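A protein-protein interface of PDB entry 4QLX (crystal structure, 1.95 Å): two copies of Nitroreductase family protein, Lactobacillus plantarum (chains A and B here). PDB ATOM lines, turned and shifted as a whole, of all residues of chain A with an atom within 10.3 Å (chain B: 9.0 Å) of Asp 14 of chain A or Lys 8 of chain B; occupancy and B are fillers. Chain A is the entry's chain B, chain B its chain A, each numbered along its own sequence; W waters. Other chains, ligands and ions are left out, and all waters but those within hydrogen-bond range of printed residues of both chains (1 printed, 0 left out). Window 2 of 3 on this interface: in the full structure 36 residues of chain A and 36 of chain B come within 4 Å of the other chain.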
ATOM      1  N   LEU A  10     -18.909   7.103  -7.530  1.00  0.00           N
ATOM      2  CA  LEU A  10     -18.456   7.103  -8.921  1.00  0.00           C
ATOM      3  C   LEU A  10     -17.070   7.708  -9.019  1.00  0.00           C
ATOM      4  O   LEU A  10     -16.859   8.857  -8.649  1.00  0.00           O
ATOM      5  CB  LEU A  10     -19.420   7.881  -9.823  1.00  0.00           C
ATOM      6  CG  LEU A  10     -20.841   7.341 -10.020  1.00  0.00           C
ATOM      7  CD1 LEU A  10     -21.587   8.184 -11.039  1.00  0.00           C
ATOM      8  CD2 LEU A  10     -20.835   5.872 -10.433  1.00  0.00           C
ATOM      9  N   VAL A  11     -16.128   6.926  -9.525  1.00  0.00           N
ATOM     10  CA  VAL A  11     -14.769   7.388  -9.728  1.00  0.00           C
ATOM     11  C   VAL A  11     -14.687   8.499 -10.769  1.00  0.00           C
ATOM     12  O   VAL A  11     -13.939   9.466 -10.613  1.00  0.00           O
ATOM     13  CB  VAL A  11     -13.863   6.236 -10.186  1.00  0.00           C
ATOM     14  CG1 VAL A  11     -12.417   6.692 -10.219  1.00  0.00           C
ATOM     15  CG2 VAL A  11     -14.027   5.042  -9.264  1.00  0.00           C
ATOM     16  N   ASN A  12     -15.437   8.331 -11.851  1.00  0.00           N
ATOM     17  CA  ASN A  12     -15.430   9.288 -12.942  1.00  0.00           C
ATOM     18  C   ASN A  12     -16.861   9.722 -13.249  1.00  0.00           C
ATOM     19  O   ASN A  12     -17.624   8.996 -13.888  1.00  0.00           O
ATOM     20  CB  ASN A  12     -14.754   8.685 -14.172  1.00  0.00           C
ATOM     21  CG  ASN A  12     -14.568   9.684 -15.294  1.00  0.00           C
ATOM     22  OD1 ASN A  12     -14.937  10.855 -15.181  1.00  0.00           O
ATOM     23  ND2 ASN A  12     -13.969   9.228 -16.384  1.00  0.00           N
ATOM     24  N   ASN A  13     -17.219  10.911 -12.782  1.00  0.00           N
ATOM     25  CA  ASN A  13     -18.573  11.420 -12.951  1.00  0.00           C
ATOM     26  C   ASN A  13     -18.610  12.513 -14.025  1.00  0.00           C
ATOM     27  O   ASN A  13     -19.584  13.252 -14.139  1.00  0.00           O
ATOM     28  CB  ASN A  13     -19.113  11.960 -11.624  1.00  0.00           C
ATOM     29  CG  ASN A  13     -20.619  12.181 -11.658  1.00  0.00           C
ATOM     30  OD1 ASN A  13     -21.367  11.324 -12.120  1.00  0.00           O
ATOM     31  ND2 ASN A  13     -21.062  13.348 -11.199  1.00  0.00           N
ATOM     32  N   ASP A  14     -17.532  12.616 -14.795  1.00  0.00           N
ATOM     33  CA  ASP A  14     -17.446  13.558 -15.907  1.00  0.00           C
ATOM     34  C   ASP A  14     -18.076  12.909 -17.138  1.00  0.00           C
ATOM     35  O   ASP A  14     -17.473  12.024 -17.737  1.00  0.00           O
ATOM     36  CB  ASP A  14     -15.980  13.933 -16.140  1.00  0.00           C
ATOM     37  CG  ASP A  14     -15.784  15.036 -17.188  1.00  0.00           C
ATOM     38  OD1 ASP A  14     -16.569  15.122 -18.152  1.00  0.00           O
ATOM     39  OD2 ASP A  14     -14.791  15.796 -17.063  1.00  0.00           O
ATOM     40  N   LEU A  15     -19.290  13.326 -17.500  1.00  0.00           N
ATOM     41  CA  LEU A  15     -20.033  12.673 -18.590  1.00  0.00           C
ATOM     42  C   LEU A  15     -19.326  12.769 -19.953  1.00  0.00           C
ATOM     43  O   LEU A  15     -19.219  11.780 -20.693  1.00  0.00           O
ATOM     44  CB  LEU A  15     -21.434  13.265 -18.713  1.00  0.00           C
ATOM     45  CG  LEU A  15     -22.313  12.757 -19.866  1.00  0.00           C
ATOM     46  CD1 LEU A  15     -22.440  11.237 -19.857  1.00  0.00           C
ATOM     47  CD2 LEU A  15     -23.685  13.393 -19.788  1.00  0.00           C
ATOM     48  N   ALA A  16     -18.858  13.969 -20.273  1.00  0.00           N
ATOM     49  CA  ALA A  16     -18.131  14.208 -21.514  1.00  0.00           C
ATOM     50  C   ALA A  16     -16.924  13.282 -21.611  1.00  0.00           C
ATOM     51  O   ALA A  16     -16.696  12.637 -22.651  1.00  0.00           O
ATOM     52  CB  ALA A  16     -17.701  15.665 -21.597  1.00  0.00           C
ATOM     53  N   ASP A  17     -16.163  13.197 -20.523  1.00  0.00           N
ATOM     54  CA  ASP A  17     -14.989  12.318 -20.490  1.00  0.00           C
ATOM     55  C   ASP A  17     -15.397  10.852 -20.616  1.00  0.00           C
ATOM     56  O   ASP A  17     -14.820  10.096 -21.407  1.00  0.00           O
ATOM     57  CB  ASP A  17     -14.176  12.514 -19.201  1.00  0.00           C
ATOM     58  CG  ASP A  17     -12.874  11.693 -19.201  1.00  0.00           C
ATOM     59  OD1 ASP A  17     -12.085  11.852 -20.146  1.00  0.00           O
ATOM     60  OD2 ASP A  17     -12.643  10.880 -18.277  1.00  0.00           O
ATOM     61  N   VAL A  18     -16.373  10.444 -19.811  1.00  0.00           N
ATOM     62  CA  VAL A  18     -16.850   9.065 -19.841  1.00  0.00           C
ATOM     63  C   VAL A  18     -17.350   8.663 -21.227  1.00  0.00           C
ATOM     64  O   VAL A  18     -16.952   7.622 -21.764  1.00  0.00           O
ATOM     65  CB  VAL A  18     -17.974   8.830 -18.807  1.00  0.00           C
ATOM     66  CG1 VAL A  18     -18.618   7.452 -19.020  1.00  0.00           C
ATOM     67  CG2 VAL A  18     -17.408   8.929 -17.383  1.00  0.00           C
ATOM     68  N   MET A  19     -18.214   9.491 -21.812  1.00  0.00           N
ATOM     69  CA  MET A  19     -18.831   9.145 -23.085  1.00  0.00           C
ATOM     70  C   MET A  19     -17.931   9.396 -24.287  1.00  0.00           C
ATOM     71  O   MET A  19     -17.867   8.566 -25.181  1.00  0.00           O
ATOM     72  CB  MET A  19     -20.125   9.917 -23.292  1.00  0.00           C
ATOM     73  CG  MET A  19     -20.895   9.457 -24.541  1.00  0.00           C
ATOM     74  SD  MET A  19     -22.436  10.377 -24.798  1.00  0.00           S
ATOM     75  CE  MET A  19     -23.388   9.816 -23.381  1.00  0.00           C
ATOM     76  N   PHE A  20     -17.270  10.549 -24.327  1.00  0.00           N
ATOM     77  CA  PHE A  20     -16.541  10.951 -25.541  1.00  0.00           C
ATOM     78  C   PHE A  20     -15.106  10.460 -25.565  1.00  0.00           C
ATOM     79  O   PHE A  20     -14.435  10.526 -26.611  1.00  0.00           O
ATOM     80  CB  PHE A  20     -16.553  12.474 -25.703  1.00  0.00           C
ATOM     81  CG  PHE A  20     -17.927  13.060 -25.777  1.00  0.00           C
ATOM     82  CD1 PHE A  20     -18.991  12.300 -26.238  1.00  0.00           C
ATOM     83  CD2 PHE A  20     -18.161  14.369 -25.386  1.00  0.00           C
ATOM     84  CE1 PHE A  20     -20.266  12.829 -26.310  1.00  0.00           C
ATOM     85  CE2 PHE A  20     -19.432  14.902 -25.452  1.00  0.00           C
ATOM     86  CZ  PHE A  20     -20.488  14.133 -25.907  1.00  0.00           C
ATOM     87  N   ASN A  21     -14.619   9.970 -24.430  1.00  0.00           N
ATOM     88  CA  ASN A  21     -13.281   9.371 -24.408  1.00  0.00           C
ATOM     89  C   ASN A  21     -13.355   7.867 -24.179  1.00  0.00           C
ATOM     90  O   ASN A  21     -12.354   7.222 -23.827  1.00  0.00           O
ATOM     91  CB  ASN A  21     -12.406  10.037 -23.350  1.00  0.00           C
ATOM     92  CG  ASN A  21     -11.980  11.436 -23.751  1.00  0.00           C
ATOM     93  OD1 ASN A  21     -11.807  11.726 -24.936  1.00  0.00           O
ATOM     94  ND2 ASN A  21     -11.793  12.305 -22.770  1.00  0.00           N
ATOM     95  N   ARG A  22     -14.554   7.324 -24.379  1.00  0.00           N
ATOM     96  CA  ARG A  22     -14.777   5.880 -24.361  1.00  0.00           C
ATOM     97  C   ARG A  22     -14.162   5.227 -25.609  1.00  0.00           C
ATOM     98  O   ARG A  22     -14.445   5.637 -26.731  1.00  0.00           O
ATOM     99  CB  ARG A  22     -16.280   5.553 -24.292  1.00  0.00           C
ATOM    100  CG  ARG A  22     -16.579   4.046 -24.250  1.00  0.00           C
ATOM    101  CD  ARG A  22     -17.941   3.690 -24.877  1.00  0.00           C
ATOM    102  NE  ARG A  22     -18.024   4.140 -26.261  1.00  0.00           N
ATOM    103  CZ  ARG A  22     -17.424   3.530 -27.282  1.00  0.00           C
ATOM    104  NH1 ARG A  22     -16.726   2.423 -27.084  1.00  0.00           N
ATOM    105  NH2 ARG A  22     -17.534   4.021 -28.505  1.00  0.00           N
ATOM    106  N   LEU A 157     -20.828   2.643 -20.347  1.00  0.00           N
ATOM    107  CA  LEU A 157     -20.607   3.934 -19.714  1.00  0.00           C
ATOM    108  C   LEU A 157     -20.451   3.780 -18.197  1.00  0.00           C
ATOM    109  O   LEU A 157     -19.579   4.406 -17.596  1.00  0.00           O
ATOM    110  CB  LEU A 157     -21.764   4.904 -20.036  1.00  0.00           C
ATOM    111  CG  LEU A 157     -21.956   5.236 -21.519  1.00  0.00           C
ATOM    112  CD1 LEU A 157     -23.212   6.109 -21.760  1.00  0.00           C
ATOM    113  CD2 LEU A 157     -20.715   5.919 -22.120  1.00  0.00           C
ATOM    114  N   VAL A 158     -21.311   2.972 -17.580  1.00  0.00           N
ATOM    115  CA  VAL A 158     -21.189   2.711 -16.141  1.00  0.00           C
ATOM    116  C   VAL A 158     -19.804   2.119 -15.769  1.00  0.00           C
ATOM    117  O   VAL A 158     -19.226   2.463 -14.730  1.00  0.00           O
ATOM    118  CB  VAL A 158     -22.325   1.784 -15.659  1.00  0.00           C
ATOM    119  CG1 VAL A 158     -22.073   1.314 -14.221  1.00  0.00           C
ATOM    120  CG2 VAL A 158     -23.669   2.525 -15.720  1.00  0.00           C
ATOM    121  N   ARG A 160     -16.888   2.764 -17.167  1.00  0.00           N
ATOM    122  CA  ARG A 160     -15.944   3.869 -17.105  1.00  0.00           C
ATOM    123  C   ARG A 160     -16.221   4.813 -15.933  1.00  0.00           C
ATOM    124  O   ARG A 160     -15.290   5.389 -15.361  1.00  0.00           O
ATOM    125  CB  ARG A 160     -15.942   4.649 -18.423  1.00  0.00           C
ATOM    126  CG  ARG A 160     -15.206   3.902 -19.546  1.00  0.00           C
ATOM    127  CD  ARG A 160     -15.253   4.652 -20.881  1.00  0.00           C
ATOM    128  NE  ARG A 160     -14.835   6.059 -20.804  1.00  0.00           N
ATOM    129  CZ  ARG A 160     -13.613   6.479 -20.473  1.00  0.00           C
ATOM    130  NH1 ARG A 160     -12.645   5.624 -20.145  1.00  0.00           N
ATOM    131  NH2 ARG A 160     -13.363   7.779 -20.459  1.00  0.00           N
ATOM    132  N   ALA A 161     -17.489   4.987 -15.575  1.00  0.00           N
ATOM    133  CA  ALA A 161     -17.811   5.832 -14.433  1.00  0.00           C
ATOM    134  C   ALA A 161     -17.189   5.255 -13.150  1.00  0.00           C
ATOM    135  O   ALA A 161     -16.849   5.993 -12.203  1.00  0.00           O
ATOM    136  CB  ALA A 161     -19.328   5.983 -14.286  1.00  0.00           C
ATOM    137  N   HIS A 162     -17.048   3.931 -13.145  1.00  0.00           N
ATOM    138  CA  HIS A 162     -16.456   3.170 -12.044  1.00  0.00           C
ATOM    139  C   HIS A 162     -14.931   3.060 -12.152  1.00  0.00           C
ATOM    140  O   HIS A 162     -14.289   2.387 -11.339  1.00  0.00           O
ATOM    141  CB  HIS A 162     -17.072   1.762 -11.997  1.00  0.00           C
ATOM    142  CG  HIS A 162     -18.392   1.703 -11.292  1.00  0.00           C
ATOM    143  ND1 HIS A 162     -18.555   1.110 -10.056  1.00  0.00           N
ATOM    144  CD2 HIS A 162     -19.614   2.170 -11.645  1.00  0.00           C
ATOM    145  CE1 HIS A 162     -19.815   1.218  -9.677  1.00  0.00           C
ATOM    146  NE2 HIS A 162     -20.480   1.857 -10.624  1.00  0.00           N
ATOM    147  N   GLY A 163     -14.348   3.708 -13.156  1.00  0.00           N
ATOM    148  CA  GLY A 163     -12.904   3.666 -13.338  1.00  0.00           C
ATOM    149  C   GLY A 163     -12.375   2.502 -14.170  1.00  0.00           C
ATOM    150  O   GLY A 163     -11.155   2.276 -14.243  1.00  0.00           O
ATOM    151  N   MET B   3     -20.615  29.232 -18.628  1.00  0.00           N
ATOM    152  CA  MET B   3     -20.262  28.291 -17.562  1.00  0.00           C
ATOM    153  C   MET B   3     -19.253  27.234 -18.073  1.00  0.00           C
ATOM    154  O   MET B   3     -19.064  27.105 -19.277  1.00  0.00           O
ATOM    155  CB  MET B   3     -21.531  27.653 -17.001  1.00  0.00           C
ATOM    156  CG  MET B   3     -21.317  26.854 -15.735  1.00  0.00           C
ATOM    157  SD  MET B   3     -22.221  25.325 -15.876  1.00  0.00           S
ATOM    158  CE  MET B   3     -21.685  24.905 -17.522  1.00  0.00           C
ATOM    159  N   SER B   4     -18.593  26.497 -17.179  1.00  0.00           N
ATOM    160  CA  SER B   4     -17.363  25.780 -17.560  1.00  0.00           C
ATOM    161  C   SER B   4     -17.546  24.535 -18.438  1.00  0.00           C
ATOM    162  O   SER B   4     -16.885  24.414 -19.468  1.00  0.00           O
ATOM    163  CB  SER B   4     -16.570  25.375 -16.311  1.00  0.00           C
ATOM    164  N   GLU B   5     -18.423  23.613 -18.042  1.00  0.00           N
ATOM    165  CA  GLU B   5     -18.497  22.308 -18.700  1.00  0.00           C
ATOM    166  C   GLU B   5     -18.978  22.449 -20.173  1.00  0.00           C
ATOM    167  O   GLU B   5     -18.998  21.481 -20.924  1.00  0.00           O
ATOM    168  CB  GLU B   5     -19.370  21.352 -17.848  1.00  0.00           C
ATOM    169  CG  GLU B   5     -20.812  21.763 -17.709  1.00  0.00           C
ATOM    170  CD  GLU B   5     -21.531  21.375 -16.407  1.00  0.00           C
ATOM    171  OE1 GLU B   5     -21.237  20.311 -15.816  1.00  0.00           O
ATOM    172  OE2 GLU B   5     -22.449  22.129 -15.995  1.00  0.00           O
ATOM    173  N   ALA B   6     -19.355  23.659 -20.580  1.00  0.00           N
ATOM    174  CA  ALA B   6     -19.254  24.045 -21.993  1.00  0.00           C
ATOM    175  C   ALA B   6     -18.231  25.188 -22.100  1.00  0.00           C
ATOM    176  O   ALA B   6     -18.541  26.310 -21.729  1.00  0.00           O
ATOM    177  CB  ALA B   6     -20.603  24.458 -22.549  1.00  0.00           C
ATOM    178  N   VAL B   7     -17.056  24.955 -22.691  1.00  0.00           N
ATOM    179  CA  VAL B   7     -16.885  24.032 -23.807  1.00  0.00           C
ATOM    180  C   VAL B   7     -16.279  22.640 -23.558  1.00  0.00           C
ATOM    181  O   VAL B   7     -15.166  22.339 -23.996  1.00  0.00           O
ATOM    182  CB  VAL B   7     -16.026  24.718 -24.903  1.00  0.00           C
ATOM    183  CG1 VAL B   7     -16.256  24.059 -26.279  1.00  0.00           C
ATOM    184  CG2 VAL B   7     -16.336  26.215 -24.952  1.00  0.00           C
ATOM    185  N   LYS B   8     -17.033  21.787 -22.875  1.00  0.00           N
ATOM    186  CA  LYS B   8     -17.051  20.380 -23.246  1.00  0.00           C
ATOM    187  C   LYS B   8     -18.324  20.273 -24.077  1.00  0.00           C
ATOM    188  O   LYS B   8     -18.655  19.221 -24.622  1.00  0.00           O
ATOM    189  CB  LYS B   8     -17.062  19.439 -22.037  1.00  0.00           C
ATOM    190  CG  LYS B   8     -15.681  19.086 -21.475  1.00  0.00           C
ATOM    191  CD  LYS B   8     -15.821  18.624 -20.024  1.00  0.00           C
ATOM    192  CE  LYS B   8     -14.491  18.233 -19.396  1.00  0.00           C
ATOM    193  NZ  LYS B   8     -14.136  16.795 -19.623  1.00  0.00           N
ATOM    194  N   ASN B   9     -19.016  21.412 -24.155  1.00  0.00           N
ATOM    195  CA  ASN B   9     -20.284  21.586 -24.859  1.00  0.00           C
ATOM    196  C   ASN B   9     -21.436  20.796 -24.213  1.00  0.00           C
ATOM    197  O   ASN B   9     -22.470  20.566 -24.841  1.00  0.00           O
ATOM    198  CB  ASN B   9     -20.146  21.219 -26.345  1.00  0.00           C
ATOM    199  CG  ASN B   9     -21.314  21.737 -27.185  1.00  0.00           C
ATOM    200  OD1 ASN B   9     -21.531  22.951 -27.278  1.00  0.00           O
ATOM    201  ND2 ASN B   9     -22.078  20.818 -27.791  1.00  0.00           N
ATOM    202  N   LEU B  10     -21.255  20.401 -22.952  1.00  0.00           N
ATOM    203  CA  LEU B  10     -22.313  19.746 -22.178  1.00  0.00           C
ATOM    204  C   LEU B  10     -22.682  20.596 -20.971  1.00  0.00           C
ATOM    205  O   LEU B  10     -21.901  20.674 -20.035  1.00  0.00           O
ATOM    206  CB  LEU B  10     -21.873  18.357 -21.713  1.00  0.00           C
ATOM    207  CG  LEU B  10     -21.436  17.361 -22.788  1.00  0.00           C
ATOM    208  CD1 LEU B  10     -21.368  15.957 -22.199  1.00  0.00           C
ATOM    209  CD2 LEU B  10     -22.385  17.393 -23.977  1.00  0.00           C
ATOM    210  N   VAL B  11     -23.856  21.226 -20.979  1.00  0.00           N
ATOM    211  CA  VAL B  11     -24.230  22.103 -19.872  1.00  0.00           C
ATOM    212  C   VAL B  11     -24.674  21.316 -18.618  1.00  0.00           C
ATOM    213  O   VAL B  11     -24.641  21.839 -17.511  1.00  0.00           O
ATOM    214  CB  VAL B  11     -25.341  23.094 -20.292  1.00  0.00           C
ATOM    215  CG1 VAL B  11     -26.678  22.389 -20.454  1.00  0.00           C
ATOM    216  CG2 VAL B  11     -25.438  24.242 -19.288  1.00  0.00           C
ATOM    217  N   ASN B  12     -25.089  20.066 -18.785  1.00  0.00           N
ATOM    218  CA  ASN B  12     -25.209  19.178 -17.642  1.00  0.00           C
ATOM    219  C   ASN B  12     -24.214  18.041 -17.844  1.00  0.00           C
ATOM    220  O   ASN B  12     -24.471  17.097 -18.586  1.00  0.00           O
ATOM    221  CB  ASN B  12     -26.644  18.658 -17.472  1.00  0.00           C
ATOM    222  CG  ASN B  12     -26.815  17.780 -16.230  1.00  0.00           C
ATOM    223  OD1 ASN B  12     -25.871  17.563 -15.469  1.00  0.00           O
ATOM    224  ND2 ASN B  12     -28.028  17.283 -16.017  1.00  0.00           N
ATOM    225  N   ASN B  13     -23.069  18.156 -17.188  1.00  0.00           N
ATOM    226  CA  ASN B  13     -21.973  17.209 -17.368  1.00  0.00           C
ATOM    227  C   ASN B  13     -21.838  16.273 -16.171  1.00  0.00           C
ATOM    228  O   ASN B  13     -20.823  15.607 -16.006  1.00  0.00           O
ATOM    229  CB  ASN B  13     -20.672  17.969 -17.610  1.00  0.00           C
ATOM    230  CG  ASN B  13     -19.568  17.086 -18.140  1.00  0.00           C
ATOM    231  OD1 ASN B  13     -19.777  16.313 -19.067  1.00  0.00           O
ATOM    232  ND2 ASN B  13     -18.393  17.178 -17.534  1.00  0.00           N
ATOM    233  N   ASP B  14     -22.881  16.238 -15.341  1.00  0.00           N
ATOM    234  CA  ASP B  14     -22.970  15.340 -14.188  1.00  0.00           C
ATOM    235  C   ASP B  14     -23.530  13.974 -14.623  1.00  0.00           C
ATOM    236  O   ASP B  14     -24.729  13.835 -14.802  1.00  0.00           O
ATOM    237  CB  ASP B  14     -23.855  15.991 -13.104  1.00  0.00           C
ATOM    238  CG  ASP B  14     -23.987  15.149 -11.837  1.00  0.00           C
ATOM    239  OD1 ASP B  14     -23.751  13.924 -11.867  1.00  0.00           O
ATOM    240  OD2 ASP B  14     -24.365  15.732 -10.789  1.00  0.00           O
ATOM    241  N   LEU B  15     -22.661  12.973 -14.777  1.00  0.00           N
ATOM    242  CA  LEU B  15     -23.077  11.671 -15.311  1.00  0.00           C
ATOM    243  C   LEU B  15     -24.203  11.024 -14.502  1.00  0.00           C
ATOM    244  O   LEU B  15     -25.185  10.545 -15.066  1.00  0.00           O
ATOM    245  CB  LEU B  15     -21.877  10.714 -15.377  1.00  0.00           C
ATOM    246  CG  LEU B  15     -22.110   9.333 -16.004  1.00  0.00           C
ATOM    247  CD1 LEU B  15     -20.869   8.875 -16.688  1.00  0.00           C
ATOM    248  CD2 LEU B  15     -22.506   8.280 -14.971  1.00  0.00           C
ATOM    249  N   ALA B  16     -24.052  11.016 -13.180  1.00  0.00           N
ATOM    250  CA  ALA B  16     -25.037  10.389 -12.310  1.00  0.00           C
ATOM    251  C   ALA B  16     -26.409  11.046 -12.477  1.00  0.00           C
ATOM    252  O   ALA B  16     -27.435  10.367 -12.611  1.00  0.00           O
ATOM    253  CB  ALA B  16     -24.577  10.455 -10.865  1.00  0.00           C
ATOM    254  N   VAL B  18     -27.405  12.910 -15.096  1.00  0.00           N
ATOM    255  CA  VAL B  18     -27.877  12.703 -16.456  1.00  0.00           C
ATOM    256  C   VAL B  18     -28.489  11.320 -16.624  1.00  0.00           C
ATOM    257  O   VAL B  18     -29.623  11.193 -17.083  1.00  0.00           O
ATOM    258  CB  VAL B  18     -26.735  12.910 -17.477  1.00  0.00           C
ATOM    259  CG1 VAL B  18     -27.142  12.381 -18.853  1.00  0.00           C
ATOM    260  CG2 VAL B  18     -26.385  14.384 -17.555  1.00  0.00           C
ATOM    261  N   LYS B  41     -25.263  18.890 -33.637  1.00  0.00           N
ATOM    262  CA  LYS B  41     -24.253  18.703 -32.609  1.00  0.00           C
ATOM    263  C   LYS B  41     -24.577  17.512 -31.691  1.00  0.00           C
ATOM    264  O   LYS B  41     -23.706  16.694 -31.400  1.00  0.00           O
ATOM    265  CB  LYS B  41     -24.104  19.979 -31.781  1.00  0.00           C
ATOM    266  CG  LYS B  41     -22.690  20.233 -31.310  1.00  0.00           C
ATOM    267  CD  LYS B  41     -21.769  20.435 -32.514  1.00  0.00           C
ATOM    268  CE  LYS B  41     -20.328  20.080 -32.185  1.00  0.00           C
ATOM    269  NZ  LYS B  41     -19.498  19.952 -33.427  1.00  0.00           N
ATOM    270  N   GLU B  45     -22.586  14.001 -31.298  1.00  0.00           N
ATOM    271  CA  GLU B  45     -22.160  13.542 -29.974  1.00  0.00           C
ATOM    272  C   GLU B  45     -22.641  12.113 -29.657  1.00  0.00           C
ATOM    273  O   GLU B  45     -21.877  11.290 -29.140  1.00  0.00           O
ATOM    274  CB  GLU B  45     -22.641  14.525 -28.912  1.00  0.00           C
ATOM    275  CG  GLU B  45     -21.831  15.821 -28.908  1.00  0.00           C
ATOM    276  CD  GLU B  45     -22.477  16.953 -28.118  1.00  0.00           C
ATOM    277  OE1 GLU B  45     -23.628  16.796 -27.639  1.00  0.00           O
ATOM    278  OE2 GLU B  45     -21.831  18.016 -27.984  1.00  0.00           O
ATOM    279  N   ALA B 161     -27.762  16.038 -21.250  1.00  0.00           N
ATOM    280  CA  ALA B 161     -26.517  16.771 -21.089  1.00  0.00           C
ATOM    281  C   ALA B 161     -26.589  18.170 -21.697  1.00  0.00           C
ATOM    282  O   ALA B 161     -25.837  19.061 -21.295  1.00  0.00           O
ATOM    283  CB  ALA B 161     -25.356  15.988 -21.710  1.00  0.00           C
ATOM    284  N   HIS B 162     -27.486  18.356 -22.668  1.00  0.00           N
ATOM    285  CA  HIS B 162     -27.721  19.680 -23.251  1.00  0.00           C
ATOM    286  C   HIS B 162     -28.814  20.472 -22.512  1.00  0.00           C
ATOM    287  O   HIS B 162     -29.177  21.583 -22.918  1.00  0.00           O
ATOM    288  CB  HIS B 162     -28.076  19.548 -24.730  1.00  0.00           C
ATOM    289  CG  HIS B 162     -26.887  19.295 -25.602  1.00  0.00           C
ATOM    290  ND1 HIS B 162     -26.451  20.199 -26.548  1.00  0.00           N
ATOM    291  CD2 HIS B 162     -26.026  18.247 -25.656  1.00  0.00           C
ATOM    292  CE1 HIS B 162     -25.377  19.716 -27.150  1.00  0.00           C
ATOM    293  NE2 HIS B 162     -25.102  18.533 -26.631  1.00  0.00           N
HETATM  294  O   HOH W   1     -19.167  16.191 -13.936  1.00  0.00           O
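The side-chain amino group (NZ) of Lys 8 of chain B is in salt-bridge range of the side-chain carboxylate (OD2) of Asp 14 of chain A, at 2.8 Å.
OD1 of Asp 14 of chain A lies within hydrogen-bond range of ND2 of Asn 13 of chain B.
The backbone carbonyl oxygen (O) of Asn 13 of chain B lies within hydrogen-bond range of the backbone NH (N) of Leu 15 of chain A (3.1 Å).
OD1 of Asn 13 of chain B sits at hydrogen-bond distance from N of Ala 16 of chain A (2.8 Å).
The side-chain amide nitrogen (ND2) of Asn 13 of chain A is in hydrogen-bond range of the side-chain carboxylate (OD1) of Asp 14 of chain B (2.8 Å).
The backbone NH (N) of Leu 15 of chain B sits at hydrogen-bond distance from the backbone carbonyl oxygen (O) of Asn 13 of chain A.
N of Ala 16 of chain B lies within hydrogen-bond range of OD1 of Asn 13 of chain A (2.9 Å).
The backbone carbonyl oxygen (O) of Asn 13 of chain B sits close to the backbone carbonyl oxygen (O) of Asn 13 of chain A (3.3 Å).
O of Glu 5 of chain B lies within hydrogen-bond range of N of Leu 10 of chain B (3.2 Å).
The backbone carbonyl oxygen (O) of Ala 161 of chain B is in hydrogen-bond range of the backbone NH (N) of Asn 12 of chain B, at 2.8 Å.
N of Val 11 of chain A sits at hydrogen-bond distance from O of Ala 161 of chain A.
N of Asp 14 of chain A is in hydrogen-bond range of OD1 of Asn 12 of chain A (3.2 Å).
OD1 of Asp 14 of chain A is in hydrogen-bond range of N of Asp 17 of chain A, 3.1 Å away.
The backbone carbonyl oxygen of Val 18 of chain A sits at hydrogen-bond distance from the guanidinium group of Arg 160 of chain A (2.8 Å).
Leu 10 of chain A touches Ala 16 of chain B (CD1 to CB, 3.8 Å).
Leu 15 of chain A touches Asn 12 of chain B.
Val 18 of chain B touches Leu 15 of chain A.
Leu 15 of chain A touches Ala 161 of chain B (CD2 to CB, 3.6 Å).
Lys 8 of chain B touches Ala 16 of chain A.
CB of Ala 16 of chain A touches CD1 of Leu 10 of chain B, at 3.7 Å.
CG2 of Val 18 of chain A touches CD1 of Leu 15 of chain B (3.5 Å).
Phe 20 of chain A touches Leu 10 of chain B.
CE1 of Phe 20 of chain A touches O of Glu 45 of chain B (3.6 Å).
Leu 15 of chain B touches Ala 161 of chain A (CD2 to CB, 3.98 Å).
Of the printed residues of chain B, Leu 10 of chain A touches Ala 16 (3.8 Å).
Asp 14 of chain A touches just these residues of chain B: Lys 8 (2.8 Å) and Asn 13 (2.8 Å).
Printed residues of chain B within 4 Å of Val 18 of chain A: Leu 15.
Gly 163 of chain A touches none of the printed residues of chain B.
Val 7 of chain B touches none of the printed residues of chain A.
Asn 9 of chain B touches none of the printed residues of chain A.
Leu 10 of chain B touches just these residues of chain A: Ala 16 and Phe 20.
Printed residues of chain A within 4 Å of Asn 12 of chain B: Leu 15 (3.97 Å).
Printed residues of chain A within 4 Å of Glu 45 of chain B: Phe 20 (3.6 Å).
Of the 19 printed residues of chain B, 10 touch a printed residue of chain A.
Among the printed residues, 18 pairs touch across the chains.
Among the printed residues, Asp or Glu carboxylates within 4 Å of a Lys or Arg side-chain nitrogen of the other chain: Asp 14 of chain A with Lys 8 of chain B (2.8 Å).
Asn 13 of chain A touches Asp 14 of chain B, and with the chains exchanged Asp 14 of chain A touches Asn 13 of chain B.
Asn 13 of chain A touches Ala 16 of chain B, and with the chains exchanged Ala 16 of chain A touches Asn 13 of chain B.
Leu 15 of chain A touches Asn 12 of chain B, but with the chains exchanged Asn 12 of chain A does not touch Leu 15 of chain B (4.3 Å).
Leu 15 of chain A touches Val 18 of chain B, and with the chains exchanged Val 18 of chain A touches Leu 15 of chain B.
10 positions are printed for both chains.
Of the 18 pairs that touch across the chains among the printed residues, 13 have their exchanged pair printed and touching as well.
Water W1 lies within hydrogen-bond range of the backbone carbonyl oxygen (O) of Asn 13 of chain B (2.7 Å) and the backbone carbonyl oxygen (O) of Asn 13 of chain A (3.0 Å).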
